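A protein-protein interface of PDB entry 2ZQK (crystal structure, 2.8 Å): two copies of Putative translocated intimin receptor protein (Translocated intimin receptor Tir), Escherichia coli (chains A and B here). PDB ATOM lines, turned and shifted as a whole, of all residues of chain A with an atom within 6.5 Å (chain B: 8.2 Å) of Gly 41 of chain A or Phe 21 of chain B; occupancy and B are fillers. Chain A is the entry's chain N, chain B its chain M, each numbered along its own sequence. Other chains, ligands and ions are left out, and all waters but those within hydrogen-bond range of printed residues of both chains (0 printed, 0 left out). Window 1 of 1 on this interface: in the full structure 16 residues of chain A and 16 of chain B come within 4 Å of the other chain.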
ATOM      1  N   THR A  17       3.514 -21.103   5.057  1.00  0.00           N
ATOM      2  CA  THR A  17       3.888 -20.014   4.169  1.00  0.00           C
ATOM      3  C   THR A  17       4.613 -18.948   4.979  1.00  0.00           C
ATOM      4  O   THR A  17       5.612 -18.368   4.526  1.00  0.00           O
ATOM      5  CB  THR A  17       2.663 -19.406   3.502  1.00  0.00           C
ATOM      6  OG1 THR A  17       1.987 -20.420   2.745  1.00  0.00           O
ATOM      7  CG2 THR A  17       3.077 -18.284   2.577  1.00  0.00           C
ATOM      8  N   LYS A  18       4.104 -18.700   6.183  1.00  0.00           N
ATOM      9  CA  LYS A  18       4.723 -17.731   7.069  1.00  0.00           C
ATOM     10  C   LYS A  18       6.149 -18.191   7.340  1.00  0.00           C
ATOM     11  O   LYS A  18       7.083 -17.394   7.317  1.00  0.00           O
ATOM     12  CB  LYS A  18       3.952 -17.627   8.387  1.00  0.00           C
ATOM     13  CG  LYS A  18       4.792 -17.084   9.548  1.00  0.00           C
ATOM     14  CD  LYS A  18       5.064 -18.143  10.636  1.00  0.00           C
ATOM     15  CE  LYS A  18       3.867 -18.307  11.579  1.00  0.00           C
ATOM     16  NZ  LYS A  18       4.108 -19.252  12.708  1.00  0.00           N
ATOM     17  N   PHE A  21       8.333 -17.735   4.184  1.00  0.00           N
ATOM     18  CA  PHE A  21       8.768 -16.368   4.041  1.00  0.00           C
ATOM     19  C   PHE A  21       9.905 -15.979   4.990  1.00  0.00           C
ATOM     20  O   PHE A  21      10.676 -15.061   4.704  1.00  0.00           O
ATOM     21  CB  PHE A  21       7.558 -15.458   4.222  1.00  0.00           C
ATOM     22  CG  PHE A  21       6.862 -15.138   2.943  1.00  0.00           C
ATOM     23  CD1 PHE A  21       5.483 -15.077   2.885  1.00  0.00           C
ATOM     24  CD2 PHE A  21       7.590 -14.871   1.800  1.00  0.00           C
ATOM     25  CE1 PHE A  21       4.829 -14.753   1.705  1.00  0.00           C
ATOM     26  CE2 PHE A  21       6.952 -14.543   0.618  1.00  0.00           C
ATOM     27  CZ  PHE A  21       5.564 -14.485   0.574  1.00  0.00           C
ATOM     28  N   GLN A  22      10.012 -16.677   6.116  1.00  0.00           N
ATOM     29  CA  GLN A  22      11.070 -16.392   7.078  1.00  0.00           C
ATOM     30  C   GLN A  22      12.441 -16.727   6.521  1.00  0.00           C
ATOM     31  O   GLN A  22      13.446 -16.272   7.043  1.00  0.00           O
ATOM     32  CB  GLN A  22      10.838 -17.176   8.352  1.00  0.00           C
ATOM     33  CG  GLN A  22       9.773 -16.589   9.227  1.00  0.00           C
ATOM     34  CD  GLN A  22       9.160 -17.618  10.139  1.00  0.00           C
ATOM     35  OE1 GLN A  22       9.743 -18.672  10.380  1.00  0.00           O
ATOM     36  NE2 GLN A  22       7.975 -17.321  10.658  1.00  0.00           N
ATOM     37  N   GLN A  27      12.088 -16.967  -1.146  1.00  0.00           N
ATOM     38  CA  GLN A  27      11.451 -15.824  -1.778  1.00  0.00           C
ATOM     39  C   GLN A  27      12.108 -15.296  -3.057  1.00  0.00           C
ATOM     40  O   GLN A  27      13.333 -15.213  -3.166  1.00  0.00           O
ATOM     41  CB  GLN A  27      11.341 -14.691  -0.769  1.00  0.00           C
ATOM     42  CG  GLN A  27      10.226 -13.713  -1.068  1.00  0.00           C
ATOM     43  CD  GLN A  27      10.240 -12.531  -0.124  1.00  0.00           C
ATOM     44  OE1 GLN A  27      10.551 -12.676   1.063  1.00  0.00           O
ATOM     45  NE2 GLN A  27       9.892 -11.355  -0.642  1.00  0.00           N
ATOM     46  N   LYS A  28      11.263 -14.938  -4.024  1.00  0.00           N
ATOM     47  CA  LYS A  28      11.702 -14.389  -5.299  1.00  0.00           C
ATOM     48  C   LYS A  28      12.076 -12.936  -5.088  1.00  0.00           C
ATOM     49  O   LYS A  28      11.619 -12.305  -4.144  1.00  0.00           O
ATOM     50  CB  LYS A  28      10.579 -14.450  -6.331  1.00  0.00           C
ATOM     51  CG  LYS A  28      10.155 -15.850  -6.745  1.00  0.00           C
ATOM     52  CD  LYS A  28       9.257 -15.760  -7.966  1.00  0.00           C
ATOM     53  CE  LYS A  28       8.633 -17.086  -8.326  1.00  0.00           C
ATOM     54  NZ  LYS A  28       7.898 -16.963  -9.602  1.00  0.00           N
ATOM     55  N   ASN A  30      12.635  -8.932  -6.964  1.00  0.00           N
ATOM     56  CA  ASN A  30      12.322  -8.072  -8.103  1.00  0.00           C
ATOM     57  C   ASN A  30      13.538  -7.198  -8.382  1.00  0.00           C
ATOM     58  O   ASN A  30      14.573  -7.364  -7.747  1.00  0.00           O
ATOM     59  CB  ASN A  30      11.096  -7.194  -7.819  1.00  0.00           C
ATOM     60  CG  ASN A  30       9.778  -7.939  -8.021  1.00  0.00           C
ATOM     61  OD1 ASN A  30       9.728  -8.961  -8.720  1.00  0.00           O
ATOM     62  ND2 ASN A  30       8.700  -7.419  -7.428  1.00  0.00           N
ATOM     63  N   ILE A  38      15.032  -6.316  -4.718  1.00  0.00           N
ATOM     64  CA  ILE A  38      14.052  -5.860  -3.734  1.00  0.00           C
ATOM     65  C   ILE A  38      13.055  -6.968  -3.468  1.00  0.00           C
ATOM     66  O   ILE A  38      12.783  -7.794  -4.338  1.00  0.00           O
ATOM     67  CB  ILE A  38      13.228  -4.594  -4.145  1.00  0.00           C
ATOM     68  CG1 ILE A  38      12.682  -4.727  -5.566  1.00  0.00           C
ATOM     69  CG2 ILE A  38      14.050  -3.360  -3.946  1.00  0.00           C
ATOM     70  CD1 ILE A  38      11.442  -3.882  -5.809  1.00  0.00           C
ATOM     71  N   PRO A  39      12.505  -7.013  -2.250  1.00  0.00           N
ATOM     72  CA  PRO A  39      11.535  -8.062  -1.957  1.00  0.00           C
ATOM     73  C   PRO A  39      10.447  -8.029  -3.032  1.00  0.00           C
ATOM     74  O   PRO A  39      10.106  -6.965  -3.533  1.00  0.00           O
ATOM     75  CB  PRO A  39      11.029  -7.667  -0.574  1.00  0.00           C
ATOM     76  CG  PRO A  39      12.256  -7.073   0.055  1.00  0.00           C
ATOM     77  CD  PRO A  39      12.782  -6.199  -1.053  1.00  0.00           C
ATOM     78  N   SER A  40       9.918  -9.200  -3.377  1.00  0.00           N
ATOM     79  CA  SER A  40       8.888  -9.319  -4.402  1.00  0.00           C
ATOM     80  C   SER A  40       7.535  -9.657  -3.796  1.00  0.00           C
ATOM     81  O   SER A  40       6.489  -9.321  -4.355  1.00  0.00           O
ATOM     82  CB  SER A  40       9.271 -10.416  -5.374  1.00  0.00           C
ATOM     83  OG  SER A  40       9.142 -11.671  -4.730  1.00  0.00           O
ATOM     84  N   GLY A  41       7.556 -10.335  -2.653  1.00  0.00           N
ATOM     85  CA  GLY A  41       6.308 -10.700  -2.006  1.00  0.00           C
ATOM     86  C   GLY A  41       5.790 -12.046  -2.488  1.00  0.00           C
ATOM     87  O   GLY A  41       4.752 -12.545  -2.027  1.00  0.00           O
ATOM     88  N   VAL A  42       6.522 -12.644  -3.419  1.00  0.00           N
ATOM     89  CA  VAL A  42       6.136 -13.930  -3.969  1.00  0.00           C
ATOM     90  C   VAL A  42       7.112 -15.011  -3.537  1.00  0.00           C
ATOM     91  O   VAL A  42       8.314 -14.765  -3.459  1.00  0.00           O
ATOM     92  CB  VAL A  42       6.139 -13.894  -5.500  1.00  0.00           C
ATOM     93  CG1 VAL A  42       5.430 -15.127  -6.049  1.00  0.00           C
ATOM     94  CG2 VAL A  42       5.508 -12.615  -5.977  1.00  0.00           C
ATOM     95  N   LEU A  43       6.592 -16.199  -3.245  1.00  0.00           N
ATOM     96  CA  LEU A  43       7.438 -17.319  -2.861  1.00  0.00           C
ATOM     97  C   LEU A  43       7.718 -18.145  -4.104  1.00  0.00           C
ATOM     98  O   LEU A  43       6.835 -18.309  -4.961  1.00  0.00           O
ATOM     99  CB  LEU A  43       6.746 -18.198  -1.813  1.00  0.00           C
ATOM    100  CG  LEU A  43       6.854 -17.729  -0.360  1.00  0.00           C
ATOM    101  CD1 LEU A  43       6.040 -18.596   0.586  1.00  0.00           C
ATOM    102  CD2 LEU A  43       8.309 -17.739   0.023  1.00  0.00           C
ATOM    103  N   ASP B  14      -1.223 -16.146  11.685  1.00  0.00           N
ATOM    104  CA  ASP B  14      -0.555 -16.766  10.541  1.00  0.00           C
ATOM    105  C   ASP B  14      -1.029 -16.122   9.261  1.00  0.00           C
ATOM    106  O   ASP B  14      -0.232 -15.718   8.426  1.00  0.00           O
ATOM    107  CB  ASP B  14      -0.855 -18.267  10.447  1.00  0.00           C
ATOM    108  CG  ASP B  14      -0.124 -19.093  11.496  1.00  0.00           C
ATOM    109  OD1 ASP B  14       1.018 -18.734  11.872  1.00  0.00           O
ATOM    110  OD2 ASP B  14      -0.693 -20.123  11.924  1.00  0.00           O
ATOM    111  N   GLN B  15      -2.341 -16.028   9.120  1.00  0.00           N
ATOM    112  CA  GLN B  15      -2.945 -15.450   7.936  1.00  0.00           C
ATOM    113  C   GLN B  15      -2.519 -14.007   7.687  1.00  0.00           C
ATOM    114  O   GLN B  15      -2.100 -13.657   6.580  1.00  0.00           O
ATOM    115  CB  GLN B  15      -4.451 -15.518   8.058  1.00  0.00           C
ATOM    116  CG  GLN B  15      -5.177 -14.979   6.869  1.00  0.00           C
ATOM    117  CD  GLN B  15      -6.551 -14.499   7.246  1.00  0.00           C
ATOM    118  OE1 GLN B  15      -7.362 -15.260   7.790  1.00  0.00           O
ATOM    119  NE2 GLN B  15      -6.828 -13.224   6.977  1.00  0.00           N
ATOM    120  N   LEU B  16      -2.627 -13.167   8.709  1.00  0.00           N
ATOM    121  CA  LEU B  16      -2.236 -11.770   8.562  1.00  0.00           C
ATOM    122  C   LEU B  16      -0.746 -11.630   8.284  1.00  0.00           C
ATOM    123  O   LEU B  16      -0.332 -10.770   7.500  1.00  0.00           O
ATOM    124  CB  LEU B  16      -2.614 -10.978   9.808  1.00  0.00           C
ATOM    125  CG  LEU B  16      -4.128 -10.759   9.957  1.00  0.00           C
ATOM    126  CD1 LEU B  16      -4.464 -10.458  11.409  1.00  0.00           C
ATOM    127  CD2 LEU B  16      -4.589  -9.627   9.040  1.00  0.00           C
ATOM    128  N   THR B  17       0.066 -12.475   8.912  1.00  0.00           N
ATOM    129  CA  THR B  17       1.501 -12.410   8.682  1.00  0.00           C
ATOM    130  C   THR B  17       1.766 -12.774   7.243  1.00  0.00           C
ATOM    131  O   THR B  17       2.437 -12.018   6.524  1.00  0.00           O
ATOM    132  CB  THR B  17       2.276 -13.376   9.577  1.00  0.00           C
ATOM    133  OG1 THR B  17       2.108 -12.991  10.950  1.00  0.00           O
ATOM    134  CG2 THR B  17       3.762 -13.353   9.218  1.00  0.00           C
ATOM    135  N   LYS B  18       1.229 -13.928   6.824  1.00  0.00           N
ATOM    136  CA  LYS B  18       1.391 -14.409   5.451  1.00  0.00           C
ATOM    137  C   LYS B  18       0.979 -13.334   4.456  1.00  0.00           C
ATOM    138  O   LYS B  18       1.726 -13.017   3.523  1.00  0.00           O
ATOM    139  CB  LYS B  18       0.542 -15.646   5.183  1.00  0.00           C
ATOM    140  CG  LYS B  18       0.654 -16.153   3.724  1.00  0.00           C
ATOM    141  CD  LYS B  18      -0.647 -16.750   3.232  1.00  0.00           C
ATOM    142  CE  LYS B  18      -1.737 -15.699   3.248  1.00  0.00           C
ATOM    143  NZ  LYS B  18      -3.104 -16.242   3.001  1.00  0.00           N
ATOM    144  N   GLU B  19      -0.213 -12.783   4.656  1.00  0.00           N
ATOM    145  CA  GLU B  19      -0.705 -11.741   3.772  1.00  0.00           C
ATOM    146  C   GLU B  19       0.225 -10.535   3.710  1.00  0.00           C
ATOM    147  O   GLU B  19       0.549 -10.061   2.619  1.00  0.00           O
ATOM    148  CB  GLU B  19      -2.101 -11.295   4.200  1.00  0.00           C
ATOM    149  CG  GLU B  19      -3.187 -12.247   3.751  1.00  0.00           C
ATOM    150  CD  GLU B  19      -4.567 -11.874   4.253  1.00  0.00           C
ATOM    151  OE1 GLU B  19      -5.518 -12.615   3.928  1.00  0.00           O
ATOM    152  OE2 GLU B  19      -4.708 -10.854   4.965  1.00  0.00           O
ATOM    153  N   ALA B  20       0.670 -10.056   4.872  1.00  0.00           N
ATOM    154  CA  ALA B  20       1.552  -8.885   4.946  1.00  0.00           C
ATOM    155  C   ALA B  20       2.901  -9.068   4.253  1.00  0.00           C
ATOM    156  O   ALA B  20       3.532  -8.096   3.821  1.00  0.00           O
ATOM    157  CB  ALA B  20       1.760  -8.491   6.401  1.00  0.00           C
ATOM    158  N   PHE B  21       3.360 -10.305   4.149  1.00  0.00           N
ATOM    159  CA  PHE B  21       4.630 -10.541   3.484  1.00  0.00           C
ATOM    160  C   PHE B  21       4.443 -10.384   1.993  1.00  0.00           C
ATOM    161  O   PHE B  21       5.403 -10.130   1.267  1.00  0.00           O
ATOM    162  CB  PHE B  21       5.131 -11.956   3.725  1.00  0.00           C
ATOM    163  CG  PHE B  21       6.145 -12.074   4.800  1.00  0.00           C
ATOM    164  CD1 PHE B  21       5.762 -12.149   6.132  1.00  0.00           C
ATOM    165  CD2 PHE B  21       7.490 -12.171   4.484  1.00  0.00           C
ATOM    166  CE1 PHE B  21       6.716 -12.331   7.142  1.00  0.00           C
ATOM    167  CE2 PHE B  21       8.450 -12.349   5.485  1.00  0.00           C
ATOM    168  CZ  PHE B  21       8.061 -12.431   6.815  1.00  0.00           C
ATOM    169  N   GLN B  22       3.204 -10.563   1.539  1.00  0.00           N
ATOM    170  CA  GLN B  22       2.896 -10.492   0.116  1.00  0.00           C
ATOM    171  C   GLN B  22       3.029  -9.096  -0.432  1.00  0.00           C
ATOM    172  O   GLN B  22       3.060  -8.891  -1.638  1.00  0.00           O
ATOM    173  CB  GLN B  22       1.522 -11.100  -0.137  1.00  0.00           C
ATOM    174  CG  GLN B  22       1.546 -12.587   0.202  1.00  0.00           C
ATOM    175  CD  GLN B  22       0.178 -13.227   0.256  1.00  0.00           C
ATOM    176  OE1 GLN B  22      -0.775 -12.653   0.794  1.00  0.00           O
ATOM    177  NE2 GLN B  22       0.077 -14.438  -0.275  1.00  0.00           N
ATOM    178  N   ASN B  23       3.138  -8.142   0.480  1.00  0.00           N
ATOM    179  CA  ASN B  23       3.348  -6.743   0.135  1.00  0.00           C
ATOM    180  C   ASN B  23       4.790  -6.522   0.549  1.00  0.00           C
ATOM    181  O   ASN B  23       5.088  -6.302   1.725  1.00  0.00           O
ATOM    182  CB  ASN B  23       2.430  -5.850   0.951  1.00  0.00           C
ATOM    183  CG  ASN B  23       2.691  -4.394   0.703  1.00  0.00           C
ATOM    184  OD1 ASN B  23       1.926  -3.535   1.145  1.00  0.00           O
ATOM    185  ND2 ASN B  23       3.780  -4.097  -0.006  1.00  0.00           N
ATOM    186  N   PRO B  24       5.709  -6.567  -0.412  1.00  0.00           N
ATOM    187  CA  PRO B  24       7.133  -6.389  -0.134  1.00  0.00           C
ATOM    188  C   PRO B  24       7.502  -5.093   0.600  1.00  0.00           C
ATOM    189  O   PRO B  24       8.673  -4.843   0.898  1.00  0.00           O
ATOM    190  CB  PRO B  24       7.765  -6.521  -1.528  1.00  0.00           C
ATOM    191  CG  PRO B  24       6.756  -5.887  -2.404  1.00  0.00           C
ATOM    192  CD  PRO B  24       5.426  -6.375  -1.843  1.00  0.00           C
ATOM    193  N   ASP B  25       6.504  -4.275   0.909  1.00  0.00           N
ATOM    194  CA  ASP B  25       6.758  -3.024   1.606  1.00  0.00           C
ATOM    195  C   ASP B  25       6.750  -3.182   3.121  1.00  0.00           C
ATOM    196  O   ASP B  25       7.263  -2.318   3.821  1.00  0.00           O
ATOM    197  CB  ASP B  25       5.739  -1.963   1.178  1.00  0.00           C
ATOM    198  CG  ASP B  25       6.066  -1.353  -0.185  1.00  0.00           C
ATOM    199  OD1 ASP B  25       7.022  -0.553  -0.265  1.00  0.00           O
ATOM    200  OD2 ASP B  25       5.378  -1.678  -1.178  1.00  0.00           O
ATOM    201  N   ASN B  26       6.172  -4.275   3.629  1.00  0.00           N
ATOM    202  CA  ASN B  26       6.130  -4.517   5.080  1.00  0.00           C
ATOM    203  C   ASN B  26       7.324  -5.380   5.474  1.00  0.00           C
ATOM    204  O   ASN B  26       7.374  -5.928   6.573  1.00  0.00           O
ATOM    205  CB  ASN B  26       4.868  -5.283   5.501  1.00  0.00           C
ATOM    206  CG  ASN B  26       3.585  -4.647   5.013  1.00  0.00           C
ATOM    207  OD1 ASN B  26       3.432  -3.427   5.018  1.00  0.00           O
ATOM    208  ND2 ASN B  26       2.635  -5.487   4.612  1.00  0.00           N
ATOM    209  N   GLN B  27       8.294  -5.487   4.582  1.00  0.00           N
ATOM    210  CA  GLN B  27       9.429  -6.349   4.837  1.00  0.00           C
ATOM    211  C   GLN B  27      10.737  -5.672   5.125  1.00  0.00           C
ATOM    212  O   GLN B  27      11.169  -4.809   4.355  1.00  0.00           O
ATOM    213  CB  GLN B  27       9.622  -7.274   3.643  1.00  0.00           C
ATOM    214  CG  GLN B  27       9.884  -8.713   4.013  1.00  0.00           C
ATOM    215  CD  GLN B  27       9.875  -9.605   2.805  1.00  0.00           C
ATOM    216  OE1 GLN B  27       8.970  -9.526   1.962  1.00  0.00           O
ATOM    217  NE2 GLN B  27      10.876 -10.472   2.709  1.00  0.00           N
ATOM    218  N   LYS B  28      11.372  -6.071   6.230  1.00  0.00           N
ATOM    219  CA  LYS B  28      12.674  -5.521   6.586  1.00  0.00           C
ATOM    220  C   LYS B  28      13.564  -6.115   5.521  1.00  0.00           C
ATOM    221  O   LYS B  28      13.293  -7.205   5.017  1.00  0.00           O
ATOM    222  CB  LYS B  28      13.129  -5.969   7.980  1.00  0.00           C
ATOM    223  CG  LYS B  28      12.397  -5.290   9.138  1.00  0.00           C
ATOM    224  CD  LYS B  28      13.088  -5.582  10.469  1.00  0.00           C
ATOM    225  CE  LYS B  28      12.544  -4.689  11.586  1.00  0.00           C
ATOM    226  NZ  LYS B  28      13.505  -4.524  12.718  1.00  0.00           N
ATOM    227  N   PRO B  39      15.575  -9.423   0.859  1.00  0.00           N
ATOM    228  CA  PRO B  39      14.654  -9.715   1.965  1.00  0.00           C
ATOM    229  C   PRO B  39      15.306 -10.451   3.133  1.00  0.00           C
ATOM    230  O   PRO B  39      15.929 -11.493   2.952  1.00  0.00           O
ATOM    231  CB  PRO B  39      13.558 -10.543   1.292  1.00  0.00           C
ATOM    232  CG  PRO B  39      14.255 -11.157   0.097  1.00  0.00           C
ATOM    233  CD  PRO B  39      15.094 -10.016  -0.401  1.00  0.00           C
ATOM    234  N   SER B  40      15.146  -9.912   4.337  1.00  0.00           N
ATOM    235  CA  SER B  40      15.741 -10.509   5.534  1.00  0.00           C
ATOM    236  C   SER B  40      14.916 -11.645   6.128  1.00  0.00           C
ATOM    237  O   SER B  40      15.452 -12.523   6.806  1.00  0.00           O
ATOM    238  CB  SER B  40      15.964  -9.434   6.604  1.00  0.00           C
ATOM    239  OG  SER B  40      14.739  -8.817   6.975  1.00  0.00           O
ATOM    240  N   GLY B  41      13.611 -11.619   5.877  1.00  0.00           N
ATOM    241  CA  GLY B  41      12.739 -12.653   6.407  1.00  0.00           C
ATOM    242  C   GLY B  41      11.993 -12.169   7.629  1.00  0.00           C
ATOM    243  O   GLY B  41      11.290 -12.933   8.291  1.00  0.00           O
ATOM    244  N   VAL B  42      12.141 -10.880   7.918  1.00  0.00           N
ATOM    245  CA  VAL B  42      11.499 -10.275   9.071  1.00  0.00           C
ATOM    246  C   VAL B  42      10.661  -9.072   8.665  1.00  0.00           C
ATOM    247  O   VAL B  42      11.084  -8.268   7.841  1.00  0.00           O
ATOM    248  CB  VAL B  42      12.553  -9.821  10.096  1.00  0.00           C
ATOM    249  CG1 VAL B  42      11.867  -9.248  11.327  1.00  0.00           C
ATOM    250  CG2 VAL B  42      13.425 -10.986  10.490  1.00  0.00           C
ATOM    251  N   LEU B  43       9.473  -8.950   9.253  1.00  0.00           N
ATOM    252  CA  LEU B  43       8.567  -7.841   8.961  1.00  0.00           C
ATOM    253  C   LEU B  43       8.862  -6.613   9.803  1.00  0.00           C
ATOM    254  O   LEU B  43       9.418  -6.703  10.900  1.00  0.00           O
ATOM    255  CB  LEU B  43       7.126  -8.246   9.224  1.00  0.00           C
ATOM    256  CG  LEU B  43       6.479  -9.368   8.427  1.00  0.00           C
ATOM    257  CD1 LEU B  43       5.183  -9.727   9.142  1.00  0.00           C
ATOM    258  CD2 LEU B  43       6.217  -8.950   6.961  1.00  0.00           C
ATOM    259  N   LYS B  44       8.456  -5.463   9.283  1.00  0.00           N
ATOM    260  CA  LYS B  44       8.655  -4.193   9.959  1.00  0.00           C
ATOM    261  C   LYS B  44       7.928  -4.187  11.301  1.00  0.00           C
ATOM    262  O   LYS B  44       6.733  -4.483  11.363  1.00  0.00           O
ATOM    263  CB  LYS B  44       8.150  -3.070   9.054  1.00  0.00           C
ATOM    264  CG  LYS B  44       8.970  -2.925   7.775  1.00  0.00           C
ATOM    265  CD  LYS B  44       8.476  -1.785   6.907  1.00  0.00           C
ATOM    266  CE  LYS B  44       9.483  -1.463   5.816  1.00  0.00           C
ATOM    267  NZ  LYS B  44       9.097  -0.230   5.069  1.00  0.00           N
ATOM    268  N   VAL B  47       4.179  -3.543  11.628  1.00  0.00           N
ATOM    269  CA  VAL B  47       3.268  -4.588  11.197  1.00  0.00           C
ATOM    270  C   VAL B  47       3.153  -5.659  12.280  1.00  0.00           C
ATOM    271  O   VAL B  47       2.064  -5.902  12.803  1.00  0.00           O
ATOM    272  CB  VAL B  47       3.736  -5.237   9.888  1.00  0.00           C
ATOM    273  CG1 VAL B  47       2.681  -6.215   9.403  1.00  0.00           C
ATOM    274  CG2 VAL B  47       4.000  -4.159   8.835  1.00  0.00           C
ATOM    275  N   VAL B  48       4.273  -6.292  12.626  1.00  0.00           N
ATOM    276  CA  VAL B  48       4.260  -7.311  13.671  1.00  0.00           C
ATOM    277  C   VAL B  48       3.360  -6.862  14.824  1.00  0.00           C
ATOM    278  O   VAL B  48       2.446  -7.588  15.230  1.00  0.00           O
ATOM    279  CB  VAL B  48       5.668  -7.560  14.232  1.00  0.00           C
ATOM    280  CG1 VAL B  48       5.628  -8.645  15.280  1.00  0.00           C
ATOM    281  CG2 VAL B  48       6.607  -7.942  13.117  1.00  0.00           C
ATOM    282  N   ILE B  51      -0.322  -6.453  13.688  1.00  0.00           N
ATOM    283  CA  ILE B  51      -0.936  -7.753  13.443  1.00  0.00           C
ATOM    284  C   ILE B  51      -1.288  -8.388  14.790  1.00  0.00           C
ATOM    285  O   ILE B  51      -2.416  -8.855  15.006  1.00  0.00           O
ATOM    286  CB  ILE B  51       0.027  -8.693  12.696  1.00  0.00           C
ATOM    287  CG1 ILE B  51       0.244  -8.185  11.270  1.00  0.00           C
ATOM    288  CG2 ILE B  51      -0.517 -10.108  12.699  1.00  0.00           C
ATOM    289  CD1 ILE B  51       1.287  -8.949  10.505  1.00  0.00           C
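The side-chain amide oxygen (OE1) of Gln 22 of chain B lies close to the backbone carbonyl oxygen (O) of Glu 19 of chain B, at 3.4 Å.
O of Lys 18 of chain A lies close to NE2 of Gln 22 of chain A (3.5 Å).
N of Ser 40 of chain A sits close to NE2 of Gln 27 of chain A (3.5 Å).
NE2 of Gln 27 of chain A lies close to N of Gly 41 of chain A (3.2 Å).
The backbone carbonyl oxygen of Lys 28 of chain A is in hydrogen-bond range of the side-chain hydroxyl of Ser 40 of chain A, at 2.6 Å.
The backbone NH (N) of Val 42 of chain A is in hydrogen-bond range of the side-chain hydroxyl (OG) of Ser 40 of chain A.
The side-chain carboxylate (OD1) of Asp 14 of chain B is in salt-bridge range of the side-chain amino group (NZ) of Lys 18 of chain A.
The side-chain amide oxygen of Gln 27 of chain A lies within hydrogen-bond range of the side-chain amide nitrogen of Gln 27 of chain B (2.8 Å).
Thr 17 of chain A touches Lys 18 of chain B, and with the chains exchanged Lys 18 of chain A touches Thr 17 of chain B.
Gln 22 of chain A touches Gly 41 of chain B, and with the chains exchanged Gly 41 of chain A touches Gln 22 of chain B.
Gln 27 of chain B touches its own counterpart, Gln 27 of chain A.
Pro 39 of chain B touches its own counterpart, Pro 39 of chain A.
Positions printed for both chains: 17, 18, 21, 22, 27, 28, 39, 40, 41, 42 and 43.
Printed residues of chain B within 4 Å of Gly 41 of chain A: Phe 21 (3.4 Å), Gln 22 (3.5 Å) and Pro 24 (3.98 Å).
Printed residues of chain A within 4 Å of Phe 21 of chain B: Phe 21 (3.3 Å) and Gly 41 (3.4 Å).
Printed residues of chain B within 4 Å of Ser 40 of chain A: Pro 24.
Of the printed residues of chain B, Gln 22 of chain A touches Gly 41 (3.7 Å).
Of the printed residues of chain A, Thr 17 of chain B touches Lys 18 (3.9 Å).
Of the printed residues of chain B, Thr 17 of chain A touches Lys 18 (3.4 Å).
Of the printed residues of chain A, Pro 24 of chain B touches Pro 39 (3.1 Å), Ser 40 (3.9 Å) and Gly 41 (3.98 Å).
Printed residues of chain A within 4 Å of Pro 39 of chain B: Gln 27 (3.7 Å) and Pro 39 (3.9 Å).
Among the printed residues, pairs that only touch across the chains: Thr 17 of chain A with Lys 18 of chain B, Lys 18 of chain A with Thr 17 of chain B, Phe 21 of chain A with Lys 18 of chain B, Phe 21 of chain A with Phe 21 of chain B, Phe 21 of chain A with Gly 41 of chain B, Gln 22 of chain A with Gly 41 of chain B, Gln 27 of chain A with Pro 39 of chain B, Pro 39 of chain A with Pro 24 of chain B, Pro 39 of chain A with Gln 27 of chain B, Pro 39 of chain A with Pro 39 of chain B, Ser 40 of chain A with Pro 24 of chain B, Gly 41 of chain A with Phe 21 of chain B, Gly 41 of chain A with Gln 22 of chain B and Gly 41 of chain A with Pro 24 of chain B.
Of the 24 printed residues of chain B, 9 touch a printed residue of chain A.
Hydrophobic or aromatic side chains of chain B within 4 Å of the printed part of chain A: Phe 21, Pro 24 and Pro 39.
Of the 13 printed residues of chain A, 8 touch a printed residue of chain B.
Hydrophobic or aromatic side chains of chain A that line the printed part of chain B: Phe 21 and Pro 39.
Along chain A the printed residues that touch a printed residue of chain B span positions 17 to 41.
Among the printed residues, Asp or Glu carboxylates within 4 Å of a Lys or Arg side-chain nitrogen of the other chain: Lys 18 of chain A with Asp 14 of chain B (3.2 Å).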
